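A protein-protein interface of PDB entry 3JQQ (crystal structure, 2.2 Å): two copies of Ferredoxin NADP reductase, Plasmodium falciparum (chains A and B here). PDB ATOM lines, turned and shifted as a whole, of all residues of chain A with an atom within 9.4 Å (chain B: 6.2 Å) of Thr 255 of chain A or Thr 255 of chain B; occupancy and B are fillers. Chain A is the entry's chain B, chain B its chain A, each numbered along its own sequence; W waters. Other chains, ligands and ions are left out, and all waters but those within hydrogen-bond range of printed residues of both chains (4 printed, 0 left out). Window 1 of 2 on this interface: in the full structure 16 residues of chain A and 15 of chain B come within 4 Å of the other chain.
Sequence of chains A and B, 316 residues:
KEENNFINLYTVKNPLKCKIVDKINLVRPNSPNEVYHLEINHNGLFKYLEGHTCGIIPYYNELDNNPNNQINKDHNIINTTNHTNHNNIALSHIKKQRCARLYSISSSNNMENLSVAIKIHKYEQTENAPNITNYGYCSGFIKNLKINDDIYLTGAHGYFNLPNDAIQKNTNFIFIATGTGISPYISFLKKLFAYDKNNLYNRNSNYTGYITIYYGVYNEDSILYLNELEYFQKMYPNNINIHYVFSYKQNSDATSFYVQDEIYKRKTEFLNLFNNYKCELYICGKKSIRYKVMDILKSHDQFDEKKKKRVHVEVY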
ATOM      1  N   PHE A 246     -17.379  13.081  35.868  1.00  0.00           N
ATOM      2  CA  PHE A 246     -17.534  11.724  36.374  1.00  0.00           C
ATOM      3  C   PHE A 246     -18.564  10.930  35.570  1.00  0.00           C
ATOM      4  O   PHE A 246     -19.704  11.360  35.404  1.00  0.00           O
ATOM      5  CB  PHE A 246     -17.903  11.742  37.862  1.00  0.00           C
ATOM      6  CG  PHE A 246     -16.927  12.502  38.725  1.00  0.00           C
ATOM      7  CD1 PHE A 246     -15.586  12.149  38.758  1.00  0.00           C
ATOM      8  CD2 PHE A 246     -17.353  13.560  39.511  1.00  0.00           C
ATOM      9  CE1 PHE A 246     -14.690  12.846  39.551  1.00  0.00           C
ATOM     10  CE2 PHE A 246     -16.462  14.259  40.306  1.00  0.00           C
ATOM     11  CZ  PHE A 246     -15.130  13.901  40.325  1.00  0.00           C
ATOM     12  N   SER A 247     -18.161   9.763  35.076  1.00  0.00           N
ATOM     13  CA  SER A 247     -19.047   8.968  34.233  1.00  0.00           C
ATOM     14  C   SER A 247     -20.129   8.220  35.015  1.00  0.00           C
ATOM     15  O   SER A 247     -21.123   7.794  34.431  1.00  0.00           O
ATOM     16  CB  SER A 247     -18.253   8.011  33.330  1.00  0.00           C
ATOM     17  OG  SER A 247     -17.433   7.133  34.081  1.00  0.00           O
ATOM     18  N   TYR A 248     -19.953   8.069  36.327  1.00  0.00           N
ATOM     19  CA  TYR A 248     -20.962   7.380  37.135  1.00  0.00           C
ATOM     20  C   TYR A 248     -22.276   8.163  37.150  1.00  0.00           C
ATOM     21  O   TYR A 248     -23.354   7.577  37.151  1.00  0.00           O
ATOM     22  CB  TYR A 248     -20.467   7.112  38.563  1.00  0.00           C
ATOM     23  CG  TYR A 248     -20.814   8.197  39.551  1.00  0.00           C
ATOM     24  CD1 TYR A 248     -22.013   8.164  40.255  1.00  0.00           C
ATOM     25  CD2 TYR A 248     -19.944   9.252  39.789  1.00  0.00           C
ATOM     26  CE1 TYR A 248     -22.334   9.154  41.164  1.00  0.00           C
ATOM     27  CE2 TYR A 248     -20.256  10.245  40.695  1.00  0.00           C
ATOM     28  CZ  TYR A 248     -21.451  10.192  41.380  1.00  0.00           C
ATOM     29  OH  TYR A 248     -21.760  11.183  42.283  1.00  0.00           O
ATOM     30  N   LYS A 249     -22.174   9.489  37.158  1.00  0.00           N
ATOM     31  CA  LYS A 249     -23.350  10.350  37.074  1.00  0.00           C
ATOM     32  C   LYS A 249     -24.105  10.118  35.769  1.00  0.00           C
ATOM     33  O   LYS A 249     -24.898   9.184  35.660  1.00  0.00           O
ATOM     34  CB  LYS A 249     -22.949  11.822  37.183  1.00  0.00           C
ATOM     35  CG  LYS A 249     -22.677  12.288  38.603  1.00  0.00           C
ATOM     36  CD  LYS A 249     -22.041  13.668  38.616  1.00  0.00           C
ATOM     37  CE  LYS A 249     -21.722  14.108  40.037  1.00  0.00           C
ATOM     38  NZ  LYS A 249     -20.819  15.293  40.064  1.00  0.00           N
ATOM     39  N   THR A 255     -28.808   8.544  28.215  1.00  0.00           N
ATOM     40  CA  THR A 255     -27.793   9.484  27.751  1.00  0.00           C
ATOM     41  C   THR A 255     -26.442   9.265  28.422  1.00  0.00           C
ATOM     42  O   THR A 255     -26.366   8.811  29.563  1.00  0.00           O
ATOM     43  CB  THR A 255     -28.216  10.946  28.003  1.00  0.00           C
ATOM     44  OG1 THR A 255     -27.146  11.816  27.611  1.00  0.00           O
ATOM     45  CG2 THR A 255     -28.515  11.162  29.476  1.00  0.00           C
ATOM     46  N   SER A 256     -25.378   9.598  27.700  1.00  0.00           N
ATOM     47  CA  SER A 256     -24.030   9.568  28.247  1.00  0.00           C
ATOM     48  C   SER A 256     -23.465  10.982  28.269  1.00  0.00           C
ATOM     49  O   SER A 256     -23.847  11.821  27.452  1.00  0.00           O
ATOM     50  CB  SER A 256     -23.127   8.655  27.415  1.00  0.00           C
ATOM     51  OG  SER A 256     -23.483   7.293  27.585  1.00  0.00           O
ATOM     52  N   PHE A 257     -22.562  11.249  29.206  1.00  0.00           N
ATOM     53  CA  PHE A 257     -21.949  12.571  29.309  1.00  0.00           C
ATOM     54  C   PHE A 257     -20.471  12.474  29.678  1.00  0.00           C
ATOM     55  O   PHE A 257     -20.119  12.202  30.827  1.00  0.00           O
ATOM     56  CB  PHE A 257     -22.701  13.444  30.316  1.00  0.00           C
ATOM     57  CG  PHE A 257     -22.304  14.895  30.274  1.00  0.00           C
ATOM     58  CD1 PHE A 257     -22.930  15.772  29.402  1.00  0.00           C
ATOM     59  CD2 PHE A 257     -21.303  15.377  31.101  1.00  0.00           C
ATOM     60  CE1 PHE A 257     -22.571  17.110  29.357  1.00  0.00           C
ATOM     61  CE2 PHE A 257     -20.934  16.712  31.061  1.00  0.00           C
ATOM     62  CZ  PHE A 257     -21.571  17.581  30.188  1.00  0.00           C
ATOM     63  N   TYR A 258     -19.613  12.704  28.692  1.00  0.00           N
ATOM     64  CA  TYR A 258     -18.175  12.535  28.868  1.00  0.00           C
ATOM     65  C   TYR A 258     -17.440  13.877  28.825  1.00  0.00           C
ATOM     66  O   TYR A 258     -18.070  14.935  28.792  1.00  0.00           O
ATOM     67  CB  TYR A 258     -17.621  11.563  27.821  1.00  0.00           C
ATOM     68  CG  TYR A 258     -18.055  10.121  28.022  1.00  0.00           C
ATOM     69  CD1 TYR A 258     -17.814   9.465  29.222  1.00  0.00           C
ATOM     70  CD2 TYR A 258     -18.693   9.413  27.008  1.00  0.00           C
ATOM     71  CE1 TYR A 258     -18.203   8.150  29.415  1.00  0.00           C
ATOM     72  CE2 TYR A 258     -19.084   8.093  27.191  1.00  0.00           C
ATOM     73  CZ  TYR A 258     -18.835   7.467  28.397  1.00  0.00           C
ATOM     74  OH  TYR A 258     -19.217   6.155  28.592  1.00  0.00           O
ATOM     75  N   VAL A 259     -16.110  13.833  28.828  1.00  0.00           N
ATOM     76  CA  VAL A 259     -15.318  15.052  28.955  1.00  0.00           C
ATOM     77  C   VAL A 259     -15.524  16.039  27.798  1.00  0.00           C
ATOM     78  O   VAL A 259     -15.531  17.254  28.016  1.00  0.00           O
ATOM     79  CB  VAL A 259     -13.809  14.756  29.189  1.00  0.00           C
ATOM     80  CG1 VAL A 259     -13.147  14.248  27.919  1.00  0.00           C
ATOM     81  CG2 VAL A 259     -13.096  15.996  29.712  1.00  0.00           C
ATOM     82  N   GLN A 260     -15.705  15.526  26.580  1.00  0.00           N
ATOM     83  CA  GLN A 260     -15.967  16.388  25.429  1.00  0.00           C
ATOM     84  C   GLN A 260     -17.306  17.104  25.548  1.00  0.00           C
ATOM     85  O   GLN A 260     -17.463  18.222  25.063  1.00  0.00           O
ATOM     86  CB  GLN A 260     -15.963  15.599  24.115  1.00  0.00           C
ATOM     87  CG  GLN A 260     -15.070  14.384  24.095  1.00  0.00           C
ATOM     88  CD  GLN A 260     -15.747  13.171  24.688  1.00  0.00           C
ATOM     89  OE1 GLN A 260     -16.598  12.544  24.055  1.00  0.00           O
ATOM     90  NE2 GLN A 260     -15.365  12.828  25.904  1.00  0.00           N
ATOM     91  N   ASP A 261     -18.274  16.442  26.165  1.00  0.00           N
ATOM     92  CA  ASP A 261     -19.622  16.985  26.279  1.00  0.00           C
ATOM     93  C   ASP A 261     -19.633  18.148  27.261  1.00  0.00           C
ATOM     94  O   ASP A 261     -20.344  19.136  27.071  1.00  0.00           O
ATOM     95  CB  ASP A 261     -20.604  15.898  26.722  1.00  0.00           C
ATOM     96  CG  ASP A 261     -20.701  14.755  25.725  1.00  0.00           C
ATOM     97  OD1 ASP A 261     -20.534  13.588  26.136  1.00  0.00           O
ATOM     98  OD2 ASP A 261     -20.937  15.022  24.536  1.00  0.00           O
ATOM     99  N   GLU A 262     -18.834  18.012  28.314  1.00  0.00           N
ATOM    100  CA  GLU A 262     -18.645  19.073  29.288  1.00  0.00           C
ATOM    101  C   GLU A 262     -18.051  20.275  28.572  1.00  0.00           C
ATOM    102  O   GLU A 262     -18.491  21.415  28.758  1.00  0.00           O
ATOM    103  CB  GLU A 262     -17.681  18.606  30.379  1.00  0.00           C
ATOM    104  CG  GLU A 262     -18.127  18.924  31.793  1.00  0.00           C
ATOM    105  CD  GLU A 262     -18.501  20.381  31.981  1.00  0.00           C
ATOM    106  OE1 GLU A 262     -19.624  20.648  32.460  1.00  0.00           O
ATOM    107  OE2 GLU A 262     -17.675  21.254  31.644  1.00  0.00           O
ATOM    108  N   ILE A 263     -17.048  20.004  27.745  1.00  0.00           N
ATOM    109  CA  ILE A 263     -16.389  21.038  26.968  1.00  0.00           C
ATOM    110  C   ILE A 263     -17.348  21.663  25.965  1.00  0.00           C
ATOM    111  O   ILE A 263     -17.345  22.883  25.773  1.00  0.00           O
ATOM    112  CB  ILE A 263     -15.140  20.487  26.262  1.00  0.00           C
ATOM    113  CG1 ILE A 263     -14.099  20.054  27.291  1.00  0.00           C
ATOM    114  CG2 ILE A 263     -14.559  21.532  25.323  1.00  0.00           C
ATOM    115  CD1 ILE A 263     -12.874  19.394  26.690  1.00  0.00           C
ATOM    116  N   TYR A 264     -18.182  20.839  25.335  1.00  0.00           N
ATOM    117  CA  TYR A 264     -19.181  21.366  24.400  1.00  0.00           C
ATOM    118  C   TYR A 264     -20.240  22.177  25.140  1.00  0.00           C
ATOM    119  O   TYR A 264     -20.816  23.112  24.586  1.00  0.00           O
ATOM    120  CB  TYR A 264     -19.834  20.243  23.584  1.00  0.00           C
ATOM    121  CG  TYR A 264     -20.658  20.768  22.420  1.00  0.00           C
ATOM    122  CD1 TYR A 264     -20.065  21.014  21.186  1.00  0.00           C
ATOM    123  CD2 TYR A 264     -22.017  21.026  22.557  1.00  0.00           C
ATOM    124  CE1 TYR A 264     -20.807  21.499  20.120  1.00  0.00           C
ATOM    125  CE2 TYR A 264     -22.765  21.509  21.496  1.00  0.00           C
ATOM    126  CZ  TYR A 264     -22.154  21.742  20.280  1.00  0.00           C
ATOM    127  OH  TYR A 264     -22.895  22.221  19.221  1.00  0.00           O
ATOM    128  N   LYS A 265     -20.489  21.812  26.394  1.00  0.00           N
ATOM    129  CA  LYS A 265     -21.425  22.545  27.232  1.00  0.00           C
ATOM    130  C   LYS A 265     -20.945  23.979  27.428  1.00  0.00           C
ATOM    131  O   LYS A 265     -21.740  24.918  27.404  1.00  0.00           O
ATOM    132  CB  LYS A 265     -21.568  21.856  28.589  1.00  0.00           C
ATOM    133  CG  LYS A 265     -22.793  22.276  29.387  1.00  0.00           C
ATOM    134  CD  LYS A 265     -22.752  21.691  30.789  1.00  0.00           C
ATOM    135  CE  LYS A 265     -24.146  21.587  31.393  1.00  0.00           C
ATOM    136  NZ  LYS A 265     -24.840  22.906  31.445  1.00  0.00           N
ATOM    137  N   LYS A 292     -15.203  15.897  18.733  1.00  0.00           N
ATOM    138  CA  LYS A 292     -16.122  16.847  19.348  1.00  0.00           C
ATOM    139  C   LYS A 292     -15.401  18.148  19.696  1.00  0.00           C
ATOM    140  O   LYS A 292     -15.912  19.238  19.439  1.00  0.00           O
ATOM    141  CB  LYS A 292     -16.763  16.235  20.597  1.00  0.00           C
ATOM    142  CG  LYS A 292     -18.163  16.745  20.893  1.00  0.00           C
ATOM    143  CD  LYS A 292     -18.957  15.719  21.684  1.00  0.00           C
ATOM    144  CE  LYS A 292     -20.453  15.954  21.556  1.00  0.00           C
ATOM    145  NZ  LYS A 292     -21.243  14.838  22.151  1.00  0.00           N
ATOM    146  N   GLN B 250     -24.035  12.868  17.298  1.00  0.00           N
ATOM    147  CA  GLN B 250     -23.651  13.784  18.373  1.00  0.00           C
ATOM    148  C   GLN B 250     -22.557  14.769  17.943  1.00  0.00           C
ATOM    149  O   GLN B 250     -21.670  14.434  17.157  1.00  0.00           O
ATOM    150  CB  GLN B 250     -23.262  13.009  19.636  1.00  0.00           C
ATOM    151  CG  GLN B 250     -24.370  12.088  20.144  1.00  0.00           C
ATOM    152  CD  GLN B 250     -25.669  12.827  20.436  1.00  0.00           C
ATOM    153  OE1 GLN B 250     -25.760  13.589  21.400  1.00  0.00           O
ATOM    154  NE2 GLN B 250     -26.683  12.593  19.610  1.00  0.00           N
ATOM    155  N   ASN B 251     -22.640  15.985  18.477  1.00  0.00           N
ATOM    156  CA  ASN B 251     -21.878  17.135  17.982  1.00  0.00           C
ATOM    157  C   ASN B 251     -22.345  17.585  16.601  1.00  0.00           C
ATOM    158  O   ASN B 251     -23.111  18.541  16.473  1.00  0.00           O
ATOM    159  CB  ASN B 251     -20.371  16.870  17.966  1.00  0.00           C
ATOM    160  CG  ASN B 251     -19.557  18.150  17.822  1.00  0.00           C
ATOM    161  OD1 ASN B 251     -19.351  18.879  18.794  1.00  0.00           O
ATOM    162  ND2 ASN B 251     -19.089  18.425  16.606  1.00  0.00           N
ATOM    163  N   THR B 255     -23.997  16.261  24.675  1.00  0.00           N
ATOM    164  CA  THR B 255     -24.497  14.917  24.950  1.00  0.00           C
ATOM    165  C   THR B 255     -23.878  13.872  24.029  1.00  0.00           C
ATOM    166  O   THR B 255     -23.857  14.036  22.809  1.00  0.00           O
ATOM    167  CB  THR B 255     -26.037  14.853  24.813  1.00  0.00           C
ATOM    168  OG1 THR B 255     -26.647  15.393  25.986  1.00  0.00           O
ATOM    169  CG2 THR B 255     -26.494  13.414  24.638  1.00  0.00           C
ATOM    170  N   SER B 256     -23.365  12.802  24.625  1.00  0.00           N
ATOM    171  CA  SER B 256     -22.962  11.632  23.863  1.00  0.00           C
ATOM    172  C   SER B 256     -24.102  10.627  23.943  1.00  0.00           C
ATOM    173  O   SER B 256     -24.821  10.584  24.932  1.00  0.00           O
ATOM    174  CB  SER B 256     -21.671  11.032  24.424  1.00  0.00           C
ATOM    175  OG  SER B 256     -20.566  11.888  24.190  1.00  0.00           O
ATOM    176  N   PHE B 257     -24.284   9.836  22.889  1.00  0.00           N
ATOM    177  CA  PHE B 257     -25.347   8.834  22.867  1.00  0.00           C
ATOM    178  C   PHE B 257     -24.849   7.551  22.213  1.00  0.00           C
ATOM    179  O   PHE B 257     -24.618   7.511  21.008  1.00  0.00           O
ATOM    180  CB  PHE B 257     -26.585   9.366  22.136  1.00  0.00           C
ATOM    181  CG  PHE B 257     -27.799   8.485  22.272  1.00  0.00           C
ATOM    182  CD1 PHE B 257     -28.752   8.737  23.246  1.00  0.00           C
ATOM    183  CD2 PHE B 257     -27.988   7.404  21.425  1.00  0.00           C
ATOM    184  CE1 PHE B 257     -29.870   7.930  23.372  1.00  0.00           C
ATOM    185  CE2 PHE B 257     -29.104   6.595  21.546  1.00  0.00           C
ATOM    186  CZ  PHE B 257     -30.044   6.857  22.522  1.00  0.00           C
ATOM    187  N   ASP B 261     -27.022   3.663  25.885  1.00  0.00           N
ATOM    188  CA  ASP B 261     -28.067   4.666  26.047  1.00  0.00           C
ATOM    189  C   ASP B 261     -29.339   4.279  25.294  1.00  0.00           C
ATOM    190  O   ASP B 261     -30.448   4.596  25.726  1.00  0.00           O
ATOM    191  CB  ASP B 261     -27.555   6.030  25.583  1.00  0.00           C
ATOM    192  CG  ASP B 261     -26.289   6.451  26.312  1.00  0.00           C
ATOM    193  OD1 ASP B 261     -26.315   6.515  27.558  1.00  0.00           O
ATOM    194  OD2 ASP B 261     -25.268   6.716  25.642  1.00  0.00           O
ATOM    195  N   TYR B 264     -30.949   1.710  27.210  1.00  0.00           N
ATOM    196  CA  TYR B 264     -31.604   2.356  28.335  1.00  0.00           C
ATOM    197  C   TYR B 264     -32.937   2.973  27.924  1.00  0.00           C
ATOM    198  O   TYR B 264     -33.921   2.888  28.658  1.00  0.00           O
ATOM    199  CB  TYR B 264     -30.706   3.396  29.006  1.00  0.00           C
ATOM    200  CG  TYR B 264     -31.179   3.687  30.405  1.00  0.00           C
ATOM    201  CD1 TYR B 264     -30.853   2.837  31.454  1.00  0.00           C
ATOM    202  CD2 TYR B 264     -31.993   4.778  30.672  1.00  0.00           C
ATOM    203  CE1 TYR B 264     -31.301   3.081  32.736  1.00  0.00           C
ATOM    204  CE2 TYR B 264     -32.448   5.034  31.953  1.00  0.00           C
ATOM    205  CZ  TYR B 264     -32.098   4.181  32.980  1.00  0.00           C
ATOM    206  OH  TYR B 264     -32.546   4.430  34.258  1.00  0.00           O
ATOM    207  N   LYS B 292     -24.125   0.263  32.473  1.00  0.00           N
ATOM    208  CA  LYS B 292     -25.490   0.702  32.204  1.00  0.00           C
ATOM    209  C   LYS B 292     -26.419  -0.468  31.875  1.00  0.00           C
ATOM    210  O   LYS B 292     -27.573  -0.488  32.299  1.00  0.00           O
ATOM    211  CB  LYS B 292     -25.518   1.750  31.087  1.00  0.00           C
ATOM    212  CG  LYS B 292     -26.787   2.592  31.071  1.00  0.00           C
ATOM    213  CD  LYS B 292     -26.678   3.760  30.101  1.00  0.00           C
ATOM    214  CE  LYS B 292     -25.563   4.721  30.501  1.00  0.00           C
ATOM    215  NZ  LYS B 292     -25.832   6.110  30.014  1.00  0.00           N
HETATM  216  O   HOH W   1     -18.631  11.193  22.475  1.00  0.00           O
HETATM  217  O   HOH W   2     -28.794   6.441  30.485  1.00  0.00           O
HETATM  218  O   HOH W   3     -23.209  18.506  25.848  1.00  0.00           O
HETATM  219  O   HOH W   4     -23.784  19.459  19.100  1.00  0.00           O
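Water W3 bridges the backbone NH (N) of Thr 255 of chain B (2.7 Å) and the backbone carbonyl oxygen (O) of Asp 261 of chain A (3.2 Å). Water W1 lies within hydrogen-bond range of OG of Ser 256 of chain B (2.7 Å) and OE1 of Gln 260 of chain A (2.9 Å). Water W4 bridges O of Asn 251 of chain B and OH of Tyr 264 of chain A. Water W2 lies within hydrogen-bond range of the side-chain amino group of Lys 292 of chain B (3.0 Å) and the backbone NH of Thr 255 of chain A (3.1 Å).
Thr 255 of chain A touches Asp 261 of chain B, and with the chains exchanged Asp 261 of chain A touches Thr 255 of chain B. Ser 256 of chain B touches its own counterpart, Ser 256 of chain A. Ser 256 of chain A touches Asp 261 of chain B, and with the chains exchanged Asp 261 of chain A touches Ser 256 of chain B. Ser 256 of chain A touches Lys 292 of chain B, and with the chains exchanged Lys 292 of chain A touches Ser 256 of chain B. 6 positions are printed for both chains.
Thr 255 of chain A touches four residues of chain B. Of the printed residues of chain A, Thr 255 of chain B touches Thr 255, Ser 256, Asp 261 and Lys 292. Printed residues of chain A within 4 Å of Ser 256 of chain B: Thr 255 (3.8 Å), Ser 256 (3.0 Å), Asp 261 (2.6 Å) and Lys 292 (3.6 Å). Printed residues of chain A within 4 Å of Gln 250 of chain B: Lys 292. Of the printed residues of chain B, Tyr 264 of chain A touches Asn 251 (3.3 Å). The nearest residue of chain B that does not touch Thr 255 of chain A is Phe 257 of chain B (4.7 Å).
O of Ser 256 of chain B sits at hydrogen-bond distance from N of Ser 256 of chain A (3.0 Å). The side-chain hydroxyl of Ser 256 of chain A is in hydrogen-bond range of the side-chain carboxylate of Asp 261 of chain B, 2.7 Å away. OG of Ser 256 of chain B sits at hydrogen-bond distance from OD1 of Asp 261 of chain A (2.6 Å). OD2 of Asp 261 of chain A lies close to N of Thr 255 of chain B. The backbone NH (N) of Thr 255 of chain A sits close to the side-chain carboxylate (OD1) of Asp 261 of chain B (3.3 Å). O of Thr 255 of chain A is in hydrogen-bond range of NZ of Lys 292 of chain B, 2.8 Å away. NZ of Lys 292 of chain A lies within hydrogen-bond range of O of Thr 255 of chain B.
Thr 255 of chain B touches Thr 255 of chain A (CG2 to OG1, 3.4 Å). Thr 255 of chain A touches Ser 256 of chain B. Thr 255 of chain B touches Ser 256 of chain A (C to O, 3.99 Å). Ser 256 of chain A touches Lys 292 of chain B (OG to NZ, 3.6 Å). Asn 251 of chain B touches Tyr 264 of chain A (OD1 to CE1, 3.3 Å). Lys 292 of chain A touches Gln 250 of chain B (NZ to CB, 3.7 Å). CG of Lys 292 of chain A touches OD1 of Asn 251 of chain B (3.2 Å). Lys 292 of chain A touches Ser 256 of chain B (NZ to OG, 3.6 Å).
O of Thr 255 of chain B lies close to OE1 of Gln 250 of chain B, at 2.4 Å. OD1 of Asp 261 of chain B is in salt-bridge range of NZ of Lys 292 of chain B (2.5 Å). NZ of Lys 292 of chain A is in salt-bridge range of OD2 of Asp 261 of chain A, 2.4 Å away. The backbone NH of Tyr 258 of chain A is in hydrogen-bond range of the side-chain carboxylate of Asp 261 of chain A, at 2.9 Å.
Printed residues of chain A that touch a printed residue of chain B: Thr 255, Ser 256, Asp 261, Tyr 264 and Lys 292. Printed residues of chain B that touch a printed residue of chain A: Gln 250, Asn 251, Thr 255, Ser 256, Asp 261 and Lys 292. Among the printed residues, 15 pairs touch across the chains.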
